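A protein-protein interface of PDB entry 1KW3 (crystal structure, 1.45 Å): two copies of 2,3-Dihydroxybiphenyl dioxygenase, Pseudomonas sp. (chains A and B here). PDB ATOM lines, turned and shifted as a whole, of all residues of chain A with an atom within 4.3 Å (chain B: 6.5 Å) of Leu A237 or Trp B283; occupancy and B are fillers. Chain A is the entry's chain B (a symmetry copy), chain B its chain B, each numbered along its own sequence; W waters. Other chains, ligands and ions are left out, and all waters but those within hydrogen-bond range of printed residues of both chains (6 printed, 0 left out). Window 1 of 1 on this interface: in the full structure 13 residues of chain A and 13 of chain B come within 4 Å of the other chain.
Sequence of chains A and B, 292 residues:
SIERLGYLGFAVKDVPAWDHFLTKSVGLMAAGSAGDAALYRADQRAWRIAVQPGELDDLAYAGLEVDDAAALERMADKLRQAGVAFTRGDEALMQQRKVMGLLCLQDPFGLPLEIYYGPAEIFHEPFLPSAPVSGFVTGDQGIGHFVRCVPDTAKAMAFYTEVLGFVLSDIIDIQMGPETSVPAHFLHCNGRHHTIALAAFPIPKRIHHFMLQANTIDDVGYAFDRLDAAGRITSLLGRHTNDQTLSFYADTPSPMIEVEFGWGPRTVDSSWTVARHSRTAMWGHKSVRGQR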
ATOM      1  N   ASP A 218      30.786 -16.643  21.172  1.00  0.00           N
ATOM      2  CA  ASP A 218      30.637 -15.201  21.343  1.00  0.00           C
ATOM      3  C   ASP A 218      30.053 -14.557  20.091  1.00  0.00           C
ATOM      4  O   ASP A 218      29.295 -13.593  20.178  1.00  0.00           O
ATOM      5  CB  ASP A 218      31.960 -14.541  21.729  1.00  0.00           C
ATOM      6  CG  ASP A 218      32.373 -14.868  23.130  1.00  0.00           C
ATOM      7  OD1 ASP A 218      33.604 -14.885  23.386  1.00  0.00           O
ATOM      8  OD2 ASP A 218      31.554 -15.119  24.031  1.00  0.00           O
ATOM      9  N   VAL A 220      27.776 -15.760  18.295  1.00  0.00           N
ATOM     10  CA  VAL A 220      26.334 -15.966  18.457  1.00  0.00           C
ATOM     11  C   VAL A 220      25.756 -15.035  19.531  1.00  0.00           C
ATOM     12  O   VAL A 220      24.728 -14.395  19.318  1.00  0.00           O
ATOM     13  CB  VAL A 220      26.021 -17.440  18.775  1.00  0.00           C
ATOM     14  CG1 VAL A 220      24.532 -17.651  19.004  1.00  0.00           C
ATOM     15  CG2 VAL A 220      26.492 -18.341  17.639  1.00  0.00           C
ATOM     16  N   GLY A 221      26.418 -14.945  20.679  1.00  0.00           N
ATOM     17  CA  GLY A 221      25.956 -14.065  21.739  1.00  0.00           C
ATOM     18  C   GLY A 221      25.888 -12.608  21.314  1.00  0.00           C
ATOM     19  O   GLY A 221      24.932 -11.888  21.633  1.00  0.00           O
ATOM     20  N   TYR A 222      26.920 -12.144  20.626  1.00  0.00           N
ATOM     21  CA  TYR A 222      26.930 -10.766  20.176  1.00  0.00           C
ATOM     22  C   TYR A 222      25.822 -10.543  19.151  1.00  0.00           C
ATOM     23  O   TYR A 222      25.137  -9.516  19.175  1.00  0.00           O
ATOM     24  CB  TYR A 222      28.283 -10.432  19.581  1.00  0.00           C
ATOM     25  CG  TYR A 222      29.412 -10.127  20.549  1.00  0.00           C
ATOM     26  CD1 TYR A 222      30.651 -10.726  20.389  1.00  0.00           C
ATOM     27  CD2 TYR A 222      29.266  -9.196  21.558  1.00  0.00           C
ATOM     28  CE1 TYR A 222      31.712 -10.411  21.225  1.00  0.00           C
ATOM     29  CE2 TYR A 222      30.320  -8.878  22.401  1.00  0.00           C
ATOM     30  CZ  TYR A 222      31.526  -9.493  22.235  1.00  0.00           C
ATOM     31  OH  TYR A 222      32.581  -9.131  23.054  1.00  0.00           O
ATOM     32  N   PHE A 224      23.002 -12.082  18.907  1.00  0.00           N
ATOM     33  CA  PHE A 224      21.714 -12.080  19.579  1.00  0.00           C
ATOM     34  C   PHE A 224      21.376 -10.654  20.000  1.00  0.00           C
ATOM     35  O   PHE A 224      20.260 -10.179  19.790  1.00  0.00           O
ATOM     36  CB  PHE A 224      21.738 -12.986  20.805  1.00  0.00           C
ATOM     37  CG  PHE A 224      20.425 -13.061  21.531  1.00  0.00           C
ATOM     38  CD1 PHE A 224      20.074 -12.092  22.452  1.00  0.00           C
ATOM     39  CD2 PHE A 224      19.544 -14.101  21.296  1.00  0.00           C
ATOM     40  CE1 PHE A 224      18.873 -12.154  23.120  1.00  0.00           C
ATOM     41  CE2 PHE A 224      18.339 -14.162  21.959  1.00  0.00           C
ATOM     42  CZ  PHE A 224      18.004 -13.189  22.875  1.00  0.00           C
ATOM     43  N   ASP A 225      22.352  -9.983  20.605  1.00  0.00           N
ATOM     44  CA  ASP A 225      22.122  -8.629  21.082  1.00  0.00           C
ATOM     45  C   ASP A 225      21.848  -7.662  19.941  1.00  0.00           C
ATOM     46  O   ASP A 225      21.015  -6.775  20.089  1.00  0.00           O
ATOM     47  CB  ASP A 225      23.292  -8.137  21.920  1.00  0.00           C
ATOM     48  CG  ASP A 225      23.270  -8.663  23.326  1.00  0.00           C
ATOM     49  OD1 ASP A 225      24.184  -8.269  24.079  1.00  0.00           O
ATOM     50  OD2 ASP A 225      22.406  -9.446  23.740  1.00  0.00           O
ATOM     51  N   SER A 235      13.397 -16.471  19.192  1.00  0.00           N
ATOM     52  CA  SER A 235      13.692 -17.535  20.146  1.00  0.00           C
ATOM     53  C   SER A 235      14.838 -17.103  21.028  1.00  0.00           C
ATOM     54  O   SER A 235      15.754 -16.399  20.588  1.00  0.00           O
ATOM     55  CB  SER A 235      14.129 -18.825  19.438  1.00  0.00           C
ATOM     56  OG  SER A 235      15.537 -18.855  19.475  1.00  0.00           O
ATOM     57  N   LEU A 236      14.821 -17.533  22.280  1.00  0.00           N
ATOM     58  CA  LEU A 236      15.983 -17.348  23.129  1.00  0.00           C
ATOM     59  C   LEU A 236      17.075 -18.314  22.666  1.00  0.00           C
ATOM     60  O   LEU A 236      16.822 -19.233  21.891  1.00  0.00           O
ATOM     61  CB  LEU A 236      15.630 -17.617  24.585  1.00  0.00           C
ATOM     62  CG  LEU A 236      14.552 -16.700  25.181  1.00  0.00           C
ATOM     63  CD1 LEU A 236      14.407 -17.029  26.648  1.00  0.00           C
ATOM     64  CD2 LEU A 236      14.897 -15.232  24.991  1.00  0.00           C
ATOM     65  N   LEU A 237      18.299 -18.090  23.113  1.00  0.00           N
ATOM     66  CA  LEU A 237      19.379 -19.030  22.854  1.00  0.00           C
ATOM     67  C   LEU A 237      18.964 -20.448  23.270  1.00  0.00           C
ATOM     68  O   LEU A 237      18.283 -20.659  24.281  1.00  0.00           O
ATOM     69  CB  LEU A 237      20.648 -18.616  23.614  1.00  0.00           C
ATOM     70  CG  LEU A 237      21.353 -17.376  23.070  1.00  0.00           C
ATOM     71  CD1 LEU A 237      22.370 -16.822  24.061  1.00  0.00           C
ATOM     72  CD2 LEU A 237      22.009 -17.689  21.742  1.00  0.00           C
ATOM     73  N   GLY A 238      19.402 -21.423  22.506  1.00  0.00           N
ATOM     74  CA  GLY A 238      19.113 -22.807  22.830  1.00  0.00           C
ATOM     75  C   GLY A 238      19.989 -23.691  21.988  1.00  0.00           C
ATOM     76  O   GLY A 238      20.845 -23.233  21.244  1.00  0.00           O
ATOM     77  N   SER A 247      21.987 -21.994  18.932  1.00  0.00           N
ATOM     78  CA  SER A 247      21.543 -20.882  18.110  1.00  0.00           C
ATOM     79  C   SER A 247      20.419 -20.115  18.731  1.00  0.00           C
ATOM     80  O   SER A 247      19.849 -20.514  19.745  1.00  0.00           O
ATOM     81  CB  SER A 247      21.004 -21.411  16.774  1.00  0.00           C
ATOM     82  OG  SER A 247      19.883 -22.285  17.007  1.00  0.00           O
ATOM     83  N   PHE A 248      20.098 -18.989  18.103  1.00  0.00           N
ATOM     84  CA  PHE A 248      18.846 -18.299  18.356  1.00  0.00           C
ATOM     85  C   PHE A 248      18.224 -18.049  16.989  1.00  0.00           C
ATOM     86  O   PHE A 248      18.874 -18.179  15.947  1.00  0.00           O
ATOM     87  CB  PHE A 248      19.020 -16.963  19.078  1.00  0.00           C
ATOM     88  CG  PHE A 248      19.776 -15.955  18.272  1.00  0.00           C
ATOM     89  CD1 PHE A 248      19.109 -15.033  17.474  1.00  0.00           C
ATOM     90  CD2 PHE A 248      21.150 -15.938  18.283  1.00  0.00           C
ATOM     91  CE1 PHE A 248      19.803 -14.126  16.701  1.00  0.00           C
ATOM     92  CE2 PHE A 248      21.852 -15.029  17.513  1.00  0.00           C
ATOM     93  CZ  PHE A 248      21.177 -14.111  16.728  1.00  0.00           C
ATOM     94  N   TRP A 283      17.917 -27.943  24.938  1.00  0.00           N
ATOM     95  CA  TRP A 283      17.698 -26.942  25.995  1.00  0.00           C
ATOM     96  C   TRP A 283      17.448 -25.586  25.339  1.00  0.00           C
ATOM     97  O   TRP A 283      17.810 -25.384  24.184  1.00  0.00           O
ATOM     98  CB  TRP A 283      18.843 -26.842  27.032  1.00  0.00           C
ATOM     99  CG  TRP A 283      20.238 -26.626  26.527  1.00  0.00           C
ATOM    100  CD1 TRP A 283      21.210 -27.572  26.400  1.00  0.00           C
ATOM    101  CD2 TRP A 283      20.848 -25.376  26.172  1.00  0.00           C
ATOM    102  NE1 TRP A 283      22.376 -26.995  25.961  1.00  0.00           N
ATOM    103  CE2 TRP A 283      22.182 -25.649  25.811  1.00  0.00           C
ATOM    104  CE3 TRP A 283      20.402 -24.050  26.131  1.00  0.00           C
ATOM    105  CZ2 TRP A 283      23.068 -24.657  25.416  1.00  0.00           C
ATOM    106  CZ3 TRP A 283      21.290 -23.058  25.722  1.00  0.00           C
ATOM    107  CH2 TRP A 283      22.603 -23.372  25.370  1.00  0.00           C
ATOM    108  N   GLY A 284      16.774 -24.690  26.050  1.00  0.00           N
ATOM    109  CA  GLY A 284      16.536 -23.341  25.568  1.00  0.00           C
ATOM    110  C   GLY A 284      15.580 -23.219  24.407  1.00  0.00           C
ATOM    111  O   GLY A 284      14.625 -23.990  24.269  1.00  0.00           O
ATOM    112  N   HIS A 285      15.819 -22.204  23.578  1.00  0.00           N
ATOM    113  CA  HIS A 285      14.974 -21.900  22.422  1.00  0.00           C
ATOM    114  C   HIS A 285      13.539 -21.529  22.773  1.00  0.00           C
ATOM    115  O   HIS A 285      12.644 -21.667  21.942  1.00  0.00           O
ATOM    116  CB  HIS A 285      14.949 -23.051  21.422  1.00  0.00           C
ATOM    117  CG  HIS A 285      16.157 -23.134  20.545  1.00  0.00           C
ATOM    118  ND1 HIS A 285      16.496 -24.304  19.907  1.00  0.00           N
ATOM    119  CD2 HIS A 285      17.085 -22.219  20.171  1.00  0.00           C
ATOM    120  CE1 HIS A 285      17.584 -24.111  19.182  1.00  0.00           C
ATOM    121  NE2 HIS A 285      17.970 -22.852  19.329  1.00  0.00           N
ATOM    122  N   ILE B 217      29.103 -25.998  28.755  1.00  0.00           N
ATOM    123  CA  ILE B 217      28.100 -25.036  28.357  1.00  0.00           C
ATOM    124  C   ILE B 217      26.713 -25.703  28.420  1.00  0.00           C
ATOM    125  O   ILE B 217      25.728 -25.065  28.805  1.00  0.00           O
ATOM    126  CB  ILE B 217      28.374 -24.426  26.983  1.00  0.00           C
ATOM    127  CG1 ILE B 217      27.303 -23.392  26.714  1.00  0.00           C
ATOM    128  CG2 ILE B 217      28.294 -25.454  25.900  1.00  0.00           C
ATOM    129  CD1 ILE B 217      27.437 -21.977  27.218  1.00  0.00           C
ATOM    130  N   PHE B 224      19.454 -23.735  33.036  1.00  0.00           N
ATOM    131  CA  PHE B 224      18.582 -22.609  32.752  1.00  0.00           C
ATOM    132  C   PHE B 224      17.145 -23.107  32.651  1.00  0.00           C
ATOM    133  O   PHE B 224      16.229 -22.520  33.227  1.00  0.00           O
ATOM    134  CB  PHE B 224      18.983 -21.924  31.450  1.00  0.00           C
ATOM    135  CG  PHE B 224      18.144 -20.725  31.112  1.00  0.00           C
ATOM    136  CD1 PHE B 224      16.927 -20.875  30.473  1.00  0.00           C
ATOM    137  CD2 PHE B 224      18.572 -19.448  31.428  1.00  0.00           C
ATOM    138  CE1 PHE B 224      16.153 -19.781  30.159  1.00  0.00           C
ATOM    139  CE2 PHE B 224      17.797 -18.353  31.121  1.00  0.00           C
ATOM    140  CZ  PHE B 224      16.587 -18.519  30.483  1.00  0.00           C
ATOM    141  N   ASP B 225      16.960 -24.191  31.904  1.00  0.00           N
ATOM    142  CA  ASP B 225      15.622 -24.726  31.708  1.00  0.00           C
ATOM    143  C   ASP B 225      15.017 -25.234  33.008  1.00  0.00           C
ATOM    144  O   ASP B 225      13.823 -25.061  33.225  1.00  0.00           O
ATOM    145  CB  ASP B 225      15.620 -25.828  30.661  1.00  0.00           C
ATOM    146  CG  ASP B 225      15.642 -25.302  29.255  1.00  0.00           C
ATOM    147  OD1 ASP B 225      15.605 -26.154  28.344  1.00  0.00           O
ATOM    148  OD2 ASP B 225      15.695 -24.095  28.987  1.00  0.00           O
ATOM    149  N   LEU B 237      20.603 -15.869  29.470  1.00  0.00           N
ATOM    150  CA  LEU B 237      22.001 -16.225  29.283  1.00  0.00           C
ATOM    151  C   LEU B 237      22.801 -15.008  28.798  1.00  0.00           C
ATOM    152  O   LEU B 237      22.329 -14.195  27.994  1.00  0.00           O
ATOM    153  CB  LEU B 237      22.136 -17.372  28.270  1.00  0.00           C
ATOM    154  CG  LEU B 237      21.668 -18.736  28.771  1.00  0.00           C
ATOM    155  CD1 LEU B 237      21.492 -19.730  27.629  1.00  0.00           C
ATOM    156  CD2 LEU B 237      22.633 -19.270  29.808  1.00  0.00           C
ATOM    157  N   GLY B 238      24.025 -14.902  29.262  1.00  0.00           N
ATOM    158  CA  GLY B 238      24.890 -13.819  28.835  1.00  0.00           C
ATOM    159  C   GLY B 238      26.296 -14.126  29.266  1.00  0.00           C
ATOM    160  O   GLY B 238      26.590 -15.186  29.803  1.00  0.00           O
ATOM    161  N   ARG B 239      27.192 -13.188  28.989  1.00  0.00           N
ATOM    162  CA  ARG B 239      28.590 -13.351  29.322  1.00  0.00           C
ATOM    163  C   ARG B 239      29.103 -12.027  29.878  1.00  0.00           C
ATOM    164  O   ARG B 239      28.826 -10.967  29.327  1.00  0.00           O
ATOM    165  CB  ARG B 239      29.372 -13.795  28.081  1.00  0.00           C
ATOM    166  CG  ARG B 239      30.725 -14.386  28.398  1.00  0.00           C
ATOM    167  CD  ARG B 239      31.354 -15.142  27.252  1.00  0.00           C
ATOM    168  NE  ARG B 239      32.295 -16.130  27.765  1.00  0.00           N
ATOM    169  CZ  ARG B 239      32.782 -17.121  27.052  1.00  0.00           C
ATOM    170  NH1 ARG B 239      33.605 -17.993  27.619  1.00  0.00           N
ATOM    171  NH2 ARG B 239      32.470 -17.235  25.767  1.00  0.00           N
ATOM    172  N   HIS B 240      29.854 -12.100  30.970  1.00  0.00           N
ATOM    173  CA  HIS B 240      30.344 -10.899  31.634  1.00  0.00           C
ATOM    174  C   HIS B 240      31.567 -10.310  30.943  1.00  0.00           C
ATOM    175  O   HIS B 240      32.368 -11.021  30.345  1.00  0.00           O
ATOM    176  CB  HIS B 240      30.668 -11.221  33.087  1.00  0.00           C
ATOM    177  CG  HIS B 240      29.462 -11.312  33.974  1.00  0.00           C
ATOM    178  ND1 HIS B 240      28.676 -10.222  34.283  1.00  0.00           N
ATOM    179  CD2 HIS B 240      28.928 -12.362  34.645  1.00  0.00           C
ATOM    180  CE1 HIS B 240      27.718 -10.601  35.119  1.00  0.00           C
ATOM    181  NE2 HIS B 240      27.851 -11.890  35.352  1.00  0.00           N
ATOM    182  N   THR B 241      31.719  -8.998  31.041  1.00  0.00           N
ATOM    183  CA  THR B 241      32.859  -8.326  30.426  1.00  0.00           C
ATOM    184  C   THR B 241      34.202  -8.652  31.063  1.00  0.00           C
ATOM    185  O   THR B 241      35.199  -8.768  30.366  1.00  0.00           O
ATOM    186  CB  THR B 241      32.685  -6.808  30.545  1.00  0.00           C
ATOM    187  OG1 THR B 241      32.337  -6.485  31.894  1.00  0.00           O
ATOM    188  CG2 THR B 241      31.537  -6.285  29.675  1.00  0.00           C
ATOM    189  N   LEU B 246      30.103 -17.139  31.328  1.00  0.00           N
ATOM    190  CA  LEU B 246      28.878 -17.275  30.542  1.00  0.00           C
ATOM    191  C   LEU B 246      27.869 -17.912  31.497  1.00  0.00           C
ATOM    192  O   LEU B 246      28.029 -19.059  31.911  1.00  0.00           O
ATOM    193  CB  LEU B 246      29.130 -18.142  29.311  1.00  0.00           C
ATOM    194  CG  LEU B 246      28.123 -18.029  28.175  1.00  0.00           C
ATOM    195  CD1 LEU B 246      28.680 -18.724  26.950  1.00  0.00           C
ATOM    196  CD2 LEU B 246      26.781 -18.598  28.551  1.00  0.00           C
ATOM    197  N   THR B 280      28.409  -4.620  32.777  1.00  0.00           N
ATOM    198  CA  THR B 280      28.586  -5.965  33.309  1.00  0.00           C
ATOM    199  C   THR B 280      28.539  -7.020  32.228  1.00  0.00           C
ATOM    200  O   THR B 280      29.195  -8.038  32.355  1.00  0.00           O
ATOM    201  CB  THR B 280      27.510  -6.332  34.372  1.00  0.00           C
ATOM    202  OG1 THR B 280      26.203  -6.258  33.805  1.00  0.00           O
ATOM    203  CG2 THR B 280      27.491  -5.321  35.511  1.00  0.00           C
ATOM    204  N   ALA B 281      27.788  -6.773  31.167  1.00  0.00           N
ATOM    205  CA  ALA B 281      27.594  -7.801  30.145  1.00  0.00           C
ATOM    206  C   ALA B 281      28.306  -7.503  28.840  1.00  0.00           C
ATOM    207  O   ALA B 281      28.025  -6.504  28.194  1.00  0.00           O
ATOM    208  CB  ALA B 281      26.118  -7.983  29.878  1.00  0.00           C
ATOM    209  N   MET B 282      29.267  -8.339  28.482  1.00  0.00           N
ATOM    210  CA  MET B 282      29.823  -8.319  27.133  1.00  0.00           C
ATOM    211  C   MET B 282      28.677  -8.624  26.104  1.00  0.00           C
ATOM    212  O   MET B 282      28.581  -7.980  25.048  1.00  0.00           O
ATOM    213  CB  MET B 282      31.039  -9.262  27.030  1.00  0.00           C
ATOM    214  CG  MET B 282      30.817 -10.633  26.620  1.00  0.00           C
ATOM    215  SD  MET B 282      32.499 -11.394  26.727  1.00  0.00           S
ATOM    216  CE  MET B 282      32.786 -11.705  24.955  1.00  0.00           C
ATOM    217  N   TRP B 283      27.785  -9.570  26.422  1.00  0.00           N
ATOM    218  CA  TRP B 283      26.575  -9.825  25.621  1.00  0.00           C
ATOM    219  C   TRP B 283      25.538 -10.508  26.509  1.00  0.00           C
ATOM    220  O   TRP B 283      25.887 -11.081  27.536  1.00  0.00           O
ATOM    221  CB  TRP B 283      26.819 -10.650  24.334  1.00  0.00           C
ATOM    222  CG  TRP B 283      27.527 -11.965  24.461  1.00  0.00           C
ATOM    223  CD1 TRP B 283      28.837 -12.211  24.178  1.00  0.00           C
ATOM    224  CD2 TRP B 283      26.949 -13.232  24.810  1.00  0.00           C
ATOM    225  NE1 TRP B 283      29.116 -13.543  24.356  1.00  0.00           N
ATOM    226  CE2 TRP B 283      27.977 -14.194  24.746  1.00  0.00           C
ATOM    227  CE3 TRP B 283      25.661 -13.652  25.164  1.00  0.00           C
ATOM    228  CZ2 TRP B 283      27.763 -15.536  25.021  1.00  0.00           C
ATOM    229  CZ3 TRP B 283      25.453 -14.999  25.451  1.00  0.00           C
ATOM    230  CH2 TRP B 283      26.500 -15.918  25.378  1.00  0.00           C
ATOM    231  N   GLY B 284      24.266 -10.387  26.147  1.00  0.00           N
ATOM    232  CA  GLY B 284      23.192 -11.050  26.865  1.00  0.00           C
ATOM    233  C   GLY B 284      22.905 -10.523  28.251  1.00  0.00           C
ATOM    234  O   GLY B 284      23.053  -9.330  28.534  1.00  0.00           O
ATOM    235  N   HIS B 285      22.448 -11.425  29.119  1.00  0.00           N
ATOM    236  CA  HIS B 285      22.074 -11.092  30.494  1.00  0.00           C
ATOM    237  C   HIS B 285      20.917 -10.108  30.609  1.00  0.00           C
ATOM    238  O   HIS B 285      20.780  -9.431  31.626  1.00  0.00           O
ATOM    239  CB  HIS B 285      23.258 -10.546  31.285  1.00  0.00           C
ATOM    240  CG  HIS B 285      24.209 -11.591  31.775  1.00  0.00           C
ATOM    241  ND1 HIS B 285      25.502 -11.274  32.119  1.00  0.00           N
ATOM    242  CD2 HIS B 285      24.073 -12.920  32.006  1.00  0.00           C
ATOM    243  CE1 HIS B 285      26.126 -12.362  32.536  1.00  0.00           C
ATOM    244  NE2 HIS B 285      25.283 -13.381  32.471  1.00  0.00           N
ATOM    245  N   LYS B 286      20.060 -10.040  29.605  1.00  0.00           N
ATOM    246  CA  LYS B 286      18.904  -9.155  29.732  1.00  0.00           C
ATOM    247  C   LYS B 286      18.121  -9.526  30.977  1.00  0.00           C
ATOM    248  O   LYS B 286      17.857 -10.697  31.230  1.00  0.00           O
ATOM    249  CB  LYS B 286      17.998  -9.275  28.527  1.00  0.00           C
ATOM    250  CG  LYS B 286      16.824  -8.323  28.572  1.00  0.00           C
ATOM    251  CD  LYS B 286      16.222  -8.184  27.193  1.00  0.00           C
ATOM    252  CE  LYS B 286      15.228  -7.035  27.130  1.00  0.00           C
ATOM    253  NZ  LYS B 286      14.454  -7.093  25.857  1.00  0.00           N
HETATM  254  O   HOH W   1      34.922 -14.800  25.768  1.00  0.00           O
HETATM  255  O   HOH W   2      26.577  -7.147  23.075  1.00  0.00           O
HETATM  256  O   HOH W   3      23.019 -12.261  23.906  1.00  0.00           O
HETATM  257  O   HOH W   4      23.577  -7.230  26.739  1.00  0.00           O
HETATM  258  O   HOH W   5      13.718 -25.890  26.133  1.00  0.00           O
HETATM  259  O   HOH W   6      18.228 -22.925  28.255  1.00  0.00           O
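The indole nitrogen (NE1) of Trp B283 lies within hydrogen-bond range of the side-chain carboxylate (OD2) of Asp A218. The side-chain carboxylate of Asp A218 lies within salt-bridge range of the guanidinium group of Arg B239 (2.9 Å). The backbone NH (N) of Gly B284 is in hydrogen-bond range of the side-chain carboxylate (OD1) of Asp A225 (3.0 Å). The side-chain carboxylate (OD1) of Asp B225 is in hydrogen-bond range of the backbone NH (N) of Gly A284, 3.0 Å away.
N of His A285 is in hydrogen-bond range of O of Leu A237. N of Met B282 sits at hydrogen-bond distance from O of Arg B239 (2.8 Å). O of Trp B283 lies within hydrogen-bond range of N of Arg B239, at 2.9 Å. O of Leu B237 is in hydrogen-bond range of N of His B285, 3.0 Å away.
Asp A218 touches Met B282. CA of Gly A221 touches CD2 of Trp B283, 3.3 Å away. Met B282 touches Tyr A222. Tyr A222 touches Trp B283. Asp A225 touches Trp B283. Leu A237 touches Trp B283. Trp A283 touches Asp B225 (CA to OD1, 3.2 Å). CZ3 of Trp A283 touches CD1 of Leu B237 (3.8 Å).
Val A220 touches none of the printed residues of chain B. Printed residues of chain B within 4 Å of Asp A225: Trp B283 and Gly B284. Of chain B, only Trp B283 comes within 4 Å of Leu A237. Printed residues of chain A within 4 Å of Arg B239: Asp A218 (2.9 Å). Of chain A, only Asp A218 (2.9 Å), Gly A221 (3.3 Å), Tyr A222 (3.9 Å), Asp A225 (3.2 Å) and Leu A237 (3.8 Å) come within 4 Å of Trp B283. The nearest printed residue of chain A that does not touch Trp B283 is Val A220 (5.7 Å).
Of the 15 printed residues of chain A, 7 touch a printed residue of chain B. Of the 16 printed residues of chain B, 6 touch a printed residue of chain A. Hydrophobic or aromatic side chains of chain B that line the printed part of chain A: Leu B237, Met B282 and Trp B283. Among the printed residues, Asp or Glu carboxylates within 4 Å of a Lys or Arg side-chain nitrogen of the other chain: Asp A218 with Arg B239.
Asp A225 touches Trp B283, and with the chains exchanged Trp A283 touches Asp B225. Asp A225 touches Gly B284, and with the chains exchanged Gly A284 touches Asp B225. Leu A237 touches Trp B283, and with the chains exchanged Trp A283 touches Leu B237. Positions printed for both chains: 224, 225, 237, 238, 283, 284 and 285. Of the 12 pairs that touch across the chains among the printed residues, 6 have their exchanged pair printed and touching as well.
Water W1 lies within hydrogen-bond range of the side-chain carboxylate of Asp A218 (2.7 Å) and the guanidinium group of Arg B239 (3.5 Å). Water W5 bridges the backbone carbonyl oxygen of Gly A284 and the side-chain carboxylate of Asp B225. Water W4 lies within hydrogen-bond range of the backbone carbonyl oxygen (O) of Gly B284 (2.8 Å) and the side-chain carboxylate (OD1) of Asp A225 (2.9 Å). Water W2 lies within hydrogen-bond range of the side-chain carboxylate of Asp A225 (2.8 Å) and the backbone carbonyl oxygen of Met B282 (2.9 Å). Water W3 lies within hydrogen-bond range of the side-chain carboxylate (OD2) of Asp A225 (2.9 Å), the backbone carbonyl oxygen (O) of Gly A221 (3.0 Å) and the backbone NH (N) of Gly B284 (3.2 Å). Water W6 lies within hydrogen-bond range of the side-chain carboxylate of Asp B225 and the backbone NH of Gly A284.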
